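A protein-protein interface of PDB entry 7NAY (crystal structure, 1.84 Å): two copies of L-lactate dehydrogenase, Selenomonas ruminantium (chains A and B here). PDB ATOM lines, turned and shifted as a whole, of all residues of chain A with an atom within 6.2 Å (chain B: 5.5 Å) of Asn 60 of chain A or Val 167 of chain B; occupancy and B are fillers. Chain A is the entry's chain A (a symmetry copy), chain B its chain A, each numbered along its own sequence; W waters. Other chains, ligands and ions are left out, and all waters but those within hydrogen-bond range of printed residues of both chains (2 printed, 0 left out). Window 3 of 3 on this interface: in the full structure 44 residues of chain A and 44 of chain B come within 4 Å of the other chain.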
ATOM      1  N   THR A  30      18.833   7.129  -9.282  1.00  0.00           N
ATOM      2  CA  THR A  30      18.973   6.293  -8.065  1.00  0.00           C
ATOM      3  C   THR A  30      20.008   6.947  -7.149  1.00  0.00           C
ATOM      4  O   THR A  30      19.878   6.883  -5.927  1.00  0.00           O
ATOM      5  CB  THR A  30      19.421   4.890  -8.503  1.00  0.00           C
ATOM      6  OG1 THR A  30      18.439   4.350  -9.407  1.00  0.00           O
ATOM      7  CG2 THR A  30      19.668   3.966  -7.348  1.00  0.00           C
ATOM      8  N   THR A  53      16.011  13.764   0.634  1.00  0.00           N
ATOM      9  CA  THR A  53      15.598  12.481   0.021  1.00  0.00           C
ATOM     10  C   THR A  53      15.229  11.455   1.105  1.00  0.00           C
ATOM     11  O   THR A  53      14.987  10.292   0.772  1.00  0.00           O
ATOM     12  CB  THR A  53      16.640  11.968  -0.970  1.00  0.00           C
ATOM     13  OG1 THR A  53      17.806  11.604  -0.218  1.00  0.00           O
ATOM     14  CG2 THR A  53      16.873  13.010  -2.048  1.00  0.00           C
ATOM     15  N   SER A  54      15.090  11.898   2.339  1.00  0.00           N
ATOM     16  CA  SER A  54      14.532  11.106   3.459  1.00  0.00           C
ATOM     17  C   SER A  54      13.068  11.461   3.732  1.00  0.00           C
ATOM     18  O   SER A  54      12.497  10.975   4.724  1.00  0.00           O
ATOM     19  CB  SER A  54      15.366  11.302   4.686  1.00  0.00           C
ATOM     20  OG  SER A  54      16.703  10.924   4.412  1.00  0.00           O
ATOM     21  N   SER A  58       9.783  11.234  -1.086  1.00  0.00           N
ATOM     22  CA  SER A  58      10.982  11.042  -1.941  1.00  0.00           C
ATOM     23  C   SER A  58      11.303   9.559  -2.062  1.00  0.00           C
ATOM     24  O   SER A  58      11.190   8.849  -1.059  1.00  0.00           O
ATOM     25  CB  SER A  58      12.168  11.767  -1.387  1.00  0.00           C
ATOM     26  OG  SER A  58      13.206  11.754  -2.319  1.00  0.00           O
ATOM     27  N   THR A  59      11.780   9.133  -3.235  1.00  0.00           N
ATOM     28  CA  THR A  59      12.520   7.855  -3.334  1.00  0.00           C
ATOM     29  C   THR A  59      13.826   8.038  -2.536  1.00  0.00           C
ATOM     30  O   THR A  59      14.307   9.212  -2.350  1.00  0.00           O
ATOM     31  CB  THR A  59      12.701   7.449  -4.800  1.00  0.00           C
ATOM     32  OG1 THR A  59      13.166   8.584  -5.524  1.00  0.00           O
ATOM     33  CG2 THR A  59      11.437   6.895  -5.436  1.00  0.00           C
ATOM     34  N   ASN A  60      14.404   6.931  -2.080  1.00  0.00           N
ATOM     35  CA  ASN A  60      15.695   6.922  -1.348  1.00  0.00           C
ATOM     36  C   ASN A  60      16.846   7.162  -2.337  1.00  0.00           C
ATOM     37  O   ASN A  60      17.630   6.210  -2.663  1.00  0.00           O
ATOM     38  CB  ASN A  60      15.845   5.633  -0.559  1.00  0.00           C
ATOM     39  CG  ASN A  60      17.117   5.615   0.258  1.00  0.00           C
ATOM     40  OD1 ASN A  60      17.672   6.660   0.585  1.00  0.00           O
ATOM     41  ND2 ASN A  60      17.559   4.420   0.595  1.00  0.00           N
ATOM     42  N   ILE A  61      16.990   8.405  -2.786  1.00  0.00           N
ATOM     43  CA  ILE A  61      18.068   8.791  -3.742  1.00  0.00           C
ATOM     44  C   ILE A  61      19.347   9.022  -2.956  1.00  0.00           C
ATOM     45  O   ILE A  61      19.338   9.767  -1.984  1.00  0.00           O
ATOM     46  CB  ILE A  61      17.678   9.993  -4.591  1.00  0.00           C
ATOM     47  CG1 ILE A  61      16.425   9.677  -5.412  1.00  0.00           C
ATOM     48  CG2 ILE A  61      18.850  10.430  -5.460  1.00  0.00           C
ATOM     49  CD1 ILE A  61      15.863  10.869  -6.163  1.00  0.00           C
ATOM     50  N   LYS A  62      20.393   8.299  -3.330  1.00  0.00           N
ATOM     51  CA  LYS A  62      21.700   8.321  -2.622  1.00  0.00           C
ATOM     52  C   LYS A  62      22.522   9.504  -3.145  1.00  0.00           C
ATOM     53  O   LYS A  62      22.945   9.479  -4.340  1.00  0.00           O
ATOM     54  CB  LYS A  62      22.415   7.001  -2.879  1.00  0.00           C
ATOM     55  CG  LYS A  62      22.134   5.925  -1.853  1.00  0.00           C
ATOM     56  CD  LYS A  62      20.708   5.458  -1.790  1.00  0.00           C
ATOM     57  CE  LYS A  62      20.306   4.695  -3.033  1.00  0.00           C
ATOM     58  NZ  LYS A  62      19.127   3.881  -2.738  1.00  0.00           N
ATOM     59  N   ARG B 159      18.056   9.618   7.761  1.00  0.00           N
ATOM     60  CA  ARG B 159      19.194   9.450   6.821  1.00  0.00           C
ATOM     61  C   ARG B 159      20.370   8.781   7.547  1.00  0.00           C
ATOM     62  O   ARG B 159      20.978   7.893   6.970  1.00  0.00           O
ATOM     63  CB  ARG B 159      19.542  10.816   6.224  1.00  0.00           C
ATOM     64  CG  ARG B 159      20.688  10.787   5.227  1.00  0.00           C
ATOM     65  CD  ARG B 159      20.514   9.661   4.228  1.00  0.00           C
ATOM     66  NE  ARG B 159      19.500   9.898   3.218  1.00  0.00           N
ATOM     67  CZ  ARG B 159      19.068   8.972   2.374  1.00  0.00           C
ATOM     68  NH1 ARG B 159      19.553   7.745   2.440  1.00  0.00           N
ATOM     69  NH2 ARG B 159      18.149   9.273   1.478  1.00  0.00           N
ATOM     70  N   LEU B 161      20.403   6.723  10.093  1.00  0.00           N
ATOM     71  CA  LEU B 161      20.157   5.265  10.305  1.00  0.00           C
ATOM     72  C   LEU B 161      20.061   4.589   8.931  1.00  0.00           C
ATOM     73  O   LEU B 161      20.595   3.483   8.791  1.00  0.00           O
ATOM     74  CB  LEU B 161      18.916   5.059  11.168  1.00  0.00           C
ATOM     75  CG  LEU B 161      19.052   5.575  12.600  1.00  0.00           C
ATOM     76  CD1 LEU B 161      17.752   5.386  13.351  1.00  0.00           C
ATOM     77  CD2 LEU B 161      20.183   4.883  13.333  1.00  0.00           C
ATOM     78  N   ALA B 162      19.498   5.258   7.923  1.00  0.00           N
ATOM     79  CA  ALA B 162      19.412   4.708   6.543  1.00  0.00           C
ATOM     80  C   ALA B 162      20.828   4.424   6.038  1.00  0.00           C
ATOM     81  O   ALA B 162      21.104   3.295   5.546  1.00  0.00           O
ATOM     82  CB  ALA B 162      18.698   5.672   5.625  1.00  0.00           C
ATOM     83  N   ASP B 163      21.724   5.375   6.242  1.00  0.00           N
ATOM     84  CA  ASP B 163      23.112   5.277   5.718  1.00  0.00           C
ATOM     85  C   ASP B 163      23.879   4.223   6.525  1.00  0.00           C
ATOM     86  O   ASP B 163      24.687   3.513   5.930  1.00  0.00           O
ATOM     87  CB  ASP B 163      23.780   6.638   5.767  1.00  0.00           C
ATOM     88  CG  ASP B 163      23.341   7.611   4.692  1.00  0.00           C
ATOM     89  OD1 ASP B 163      22.608   7.211   3.768  1.00  0.00           O
ATOM     90  OD2 ASP B 163      23.750   8.769   4.778  1.00  0.00           O
ATOM     91  N   TYR B 165      22.804   1.479   8.053  1.00  0.00           N
ATOM     92  CA  TYR B 165      22.350   0.081   7.903  1.00  0.00           C
ATOM     93  C   TYR B 165      21.937  -0.249   6.473  1.00  0.00           C
ATOM     94  O   TYR B 165      21.549  -1.421   6.232  1.00  0.00           O
ATOM     95  CB  TYR B 165      21.226  -0.191   8.883  1.00  0.00           C
ATOM     96  CG  TYR B 165      21.649  -0.113  10.324  1.00  0.00           C
ATOM     97  CD1 TYR B 165      22.435  -1.106  10.888  1.00  0.00           C
ATOM     98  CD2 TYR B 165      21.295   0.959  11.105  1.00  0.00           C
ATOM     99  CE1 TYR B 165      22.782  -1.079  12.223  1.00  0.00           C
ATOM    100  CE2 TYR B 165      21.643   1.002  12.444  1.00  0.00           C
ATOM    101  CZ  TYR B 165      22.405  -0.010  13.001  1.00  0.00           C
ATOM    102  OH  TYR B 165      22.731   0.083  14.313  1.00  0.00           O
ATOM    103  N   GLN B 166      22.010   0.727   5.571  1.00  0.00           N
ATOM    104  CA  GLN B 166      21.619   0.537   4.157  1.00  0.00           C
ATOM    105  C   GLN B 166      20.158   0.091   4.149  1.00  0.00           C
ATOM    106  O   GLN B 166      19.838  -0.973   3.623  1.00  0.00           O
ATOM    107  CB  GLN B 166      22.586  -0.434   3.479  1.00  0.00           C
ATOM    108  CG  GLN B 166      23.952   0.189   3.237  1.00  0.00           C
ATOM    109  CD  GLN B 166      23.858   1.495   2.484  1.00  0.00           C
ATOM    110  OE1 GLN B 166      23.553   1.524   1.291  1.00  0.00           O
ATOM    111  NE2 GLN B 166      24.113   2.592   3.182  1.00  0.00           N
ATOM    112  N   VAL B 167      19.309   0.890   4.770  1.00  0.00           N
ATOM    113  CA  VAL B 167      17.836   0.665   4.813  1.00  0.00           C
ATOM    114  C   VAL B 167      17.176   1.937   4.277  1.00  0.00           C
ATOM    115  O   VAL B 167      17.822   2.996   4.312  1.00  0.00           O
ATOM    116  CB  VAL B 167      17.365   0.322   6.231  1.00  0.00           C
ATOM    117  CG1 VAL B 167      17.639   1.462   7.193  1.00  0.00           C
ATOM    118  CG2 VAL B 167      15.896  -0.059   6.257  1.00  0.00           C
ATOM    119  N   ASP B 168      15.952   1.829   3.772  1.00  0.00           N
ATOM    120  CA  ASP B 168      15.177   3.009   3.315  1.00  0.00           C
ATOM    121  C   ASP B 168      14.921   3.934   4.509  1.00  0.00           C
ATOM    122  O   ASP B 168      14.358   3.494   5.517  1.00  0.00           O
ATOM    123  CB  ASP B 168      13.885   2.516   2.667  1.00  0.00           C
ATOM    124  CG  ASP B 168      13.101   3.555   1.905  1.00  0.00           C
ATOM    125  OD1 ASP B 168      13.284   4.779   2.181  1.00  0.00           O
ATOM    126  OD2 ASP B 168      12.293   3.115   1.041  1.00  0.00           O
ATOM    127  N   PRO B 169      15.220   5.251   4.412  1.00  0.00           N
ATOM    128  CA  PRO B 169      14.935   6.185   5.500  1.00  0.00           C
ATOM    129  C   PRO B 169      13.436   6.214   5.846  1.00  0.00           C
ATOM    130  O   PRO B 169      13.083   6.456   7.000  1.00  0.00           O
ATOM    131  CB  PRO B 169      15.394   7.556   4.970  1.00  0.00           C
ATOM    132  CG  PRO B 169      15.467   7.377   3.470  1.00  0.00           C
ATOM    133  CD  PRO B 169      15.903   5.930   3.293  1.00  0.00           C
ATOM    134  N   LYS B 170      12.576   5.930   4.862  1.00  0.00           N
ATOM    135  CA  LYS B 170      11.110   5.901   5.083  1.00  0.00           C
ATOM    136  C   LYS B 170      10.748   4.784   6.057  1.00  0.00           C
ATOM    137  O   LYS B 170       9.714   4.906   6.678  1.00  0.00           O
ATOM    138  CB  LYS B 170      10.389   5.787   3.733  1.00  0.00           C
ATOM    139  CG  LYS B 170      10.532   7.049   2.897  1.00  0.00           C
ATOM    140  CD  LYS B 170       9.804   7.033   1.584  1.00  0.00           C
ATOM    141  CE  LYS B 170      10.261   5.902   0.701  1.00  0.00           C
ATOM    142  NZ  LYS B 170      11.670   6.016   0.270  1.00  0.00           N
ATOM    143  N   ASN B 171      11.572   3.744   6.210  1.00  0.00           N
ATOM    144  CA  ASN B 171      11.354   2.674   7.216  1.00  0.00           C
ATOM    145  C   ASN B 171      11.630   3.202   8.628  1.00  0.00           C
ATOM    146  O   ASN B 171      11.315   2.475   9.542  1.00  0.00           O
ATOM    147  CB  ASN B 171      12.261   1.453   6.981  1.00  0.00           C
ATOM    148  CG  ASN B 171      11.787   0.533   5.867  1.00  0.00           C
ATOM    149  OD1 ASN B 171      12.588   0.046   5.095  1.00  0.00           O
ATOM    150  ND2 ASN B 171      10.510   0.217   5.827  1.00  0.00           N
ATOM    151  N   ILE B 172      12.315   4.353   8.782  1.00  0.00           N
ATOM    152  CA  ILE B 172      12.695   4.860  10.124  1.00  0.00           C
ATOM    153  C   ILE B 172      11.546   5.716  10.662  1.00  0.00           C
ATOM    154  O   ILE B 172      11.315   6.816  10.130  1.00  0.00           O
ATOM    155  CB  ILE B 172      14.054   5.592  10.136  1.00  0.00           C
ATOM    156  CG1 ILE B 172      15.191   4.732   9.571  1.00  0.00           C
ATOM    157  CG2 ILE B 172      14.342   6.076  11.549  1.00  0.00           C
ATOM    158  CD1 ILE B 172      15.455   3.455  10.351  1.00  0.00           C
ATOM    159  N   CYS B 193      12.096   0.759  13.190  1.00  0.00           N
ATOM    160  CA  CYS B 193      12.536   0.532  11.808  1.00  0.00           C
ATOM    161  C   CYS B 193      11.673  -0.583  11.253  1.00  0.00           C
ATOM    162  O   CYS B 193      11.823  -1.727  11.715  1.00  0.00           O
ATOM    163  CB  CYS B 193      14.004   0.143  11.760  1.00  0.00           C
ATOM    164  SG  CYS B 193      14.523  -0.207  10.073  1.00  0.00           S
ATOM    165  N   LEU B 201      18.610  -3.723  14.795  1.00  0.00           N
ATOM    166  CA  LEU B 201      19.292  -3.700  13.483  1.00  0.00           C
ATOM    167  C   LEU B 201      20.711  -4.271  13.624  1.00  0.00           C
ATOM    168  O   LEU B 201      21.124  -5.013  12.739  1.00  0.00           O
ATOM    169  CB  LEU B 201      19.290  -2.260  12.974  1.00  0.00           C
ATOM    170  CG  LEU B 201      17.989  -1.782  12.336  1.00  0.00           C
ATOM    171  CD1 LEU B 201      17.982  -0.268  12.192  1.00  0.00           C
ATOM    172  CD2 LEU B 201      17.778  -2.446  10.987  1.00  0.00           C
HETATM  173  O   HOH W   1      19.681   3.659   2.290  1.00  0.00           O
HETATM  174  O   HOH W   2      12.936   8.672   1.317  1.00  0.00           O
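NH2 of Arg 159 of chain B is in hydrogen-bond range of OG1 of Thr 53 of chain A. OG of Ser 54 of chain A is in hydrogen-bond range of NE of Arg 159 of chain B (3.2 Å). The guanidinium group of Arg 159 of chain B is in hydrogen-bond range of the side-chain amide oxygen of Asn 60 of chain A (2.8 Å). The backbone carbonyl oxygen (O) of Ser 58 of chain A is in hydrogen-bond range of the side-chain amino group (NZ) of Lys 170 of chain B, 3.2 Å away.
The guanidinium group of Arg 159 of chain B is in salt-bridge range of the side-chain carboxylate of Asp 163 of chain B, 3.4 Å away. O of Ala 162 of chain B sits at hydrogen-bond distance from N of Val 167 of chain B (3.1 Å). The side-chain carboxylate of Asp 168 of chain B is in salt-bridge range of the side-chain amino group of Lys 170 of chain B (2.8 Å). O of Ile 61 of chain A lies within hydrogen-bond range of OG1 of Thr 53 of chain A (3.0 Å). The backbone carbonyl oxygen (O) of Asn 60 of chain A sits at hydrogen-bond distance from the side-chain amino group (NZ) of Lys 62 of chain A (2.8 Å).
Ser 54 of chain A touches Pro 169 of chain B (OG to CB, 3.7 Å). Asn 60 of chain A touches Val 167 of chain B (ND2 to O, 3.99 Å). OD1 of Asp 168 of chain B touches CB of Asn 60 of chain A, 3.8 Å away. Asn 60 of chain A touches Pro 169 of chain B. Lys 170 of chain B touches Asn 60 of chain A. Arg 159 of chain B touches Ile 61 of chain A.
Of the printed residues of chain B, Asn 60 of chain A touches Arg 159 (2.8 Å), Val 167 (3.99 Å), Asp 168 (3.8 Å), Pro 169 (3.3 Å) and Lys 170 (3.7 Å). Printed residues of chain A within 4 Å of Val 167 of chain B: Asn 60 (3.99 Å). Of the printed residues of chain B, Ser 58 of chain A touches Lys 170. Of the printed residues of chain A, Lys 170 of chain B touches Ser 58 (3.2 Å) and Asn 60 (3.7 Å). Of the printed residues of chain A, Arg 159 of chain B touches Thr 53 (2.9 Å), Ser 54 (3.2 Å), Asn 60 (2.8 Å) and Ile 61 (3.7 Å). Asn 171 of chain B touches none of the printed residues of chain A. Thr 59 of chain A touches none of the printed residues of chain B. The nearest printed residue of chain A that does not touch Val 167 of chain B is Lys 62 of chain A (7.2 Å). The nearest printed residue of chain A that does not touch Pro 169 of chain B is Thr 53 of chain A (4.001 Å).
Hydrophobic or aromatic side chains of chain B that line the printed part of chain A: Pro 169. Along chain B the printed residues that touch a printed residue of chain A span positions 159 to 170. Of the 8 printed residues of chain A, 5 touch a printed residue of chain B. Among the printed residues, 10 pairs touch across the chains. Among the printed residues, no Asp or Glu carboxylate lies within 4 Å of a Lys or Arg side-chain nitrogen of the other chain.
No position is printed for both chains.
Water W2 lies within hydrogen-bond range of the backbone carbonyl oxygen (O) of Thr 53 of chain A (2.7 Å), the backbone carbonyl oxygen (O) of Ser 58 of chain A (3.0 Å) and the side-chain amino group (NZ) of Lys 170 of chain B (3.1 Å). Water W1 bridges the side-chain amide nitrogen of Asn 60 of chain A (2.8 Å) and the backbone carbonyl oxygen of Val 167 of chain B (2.8 Å).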
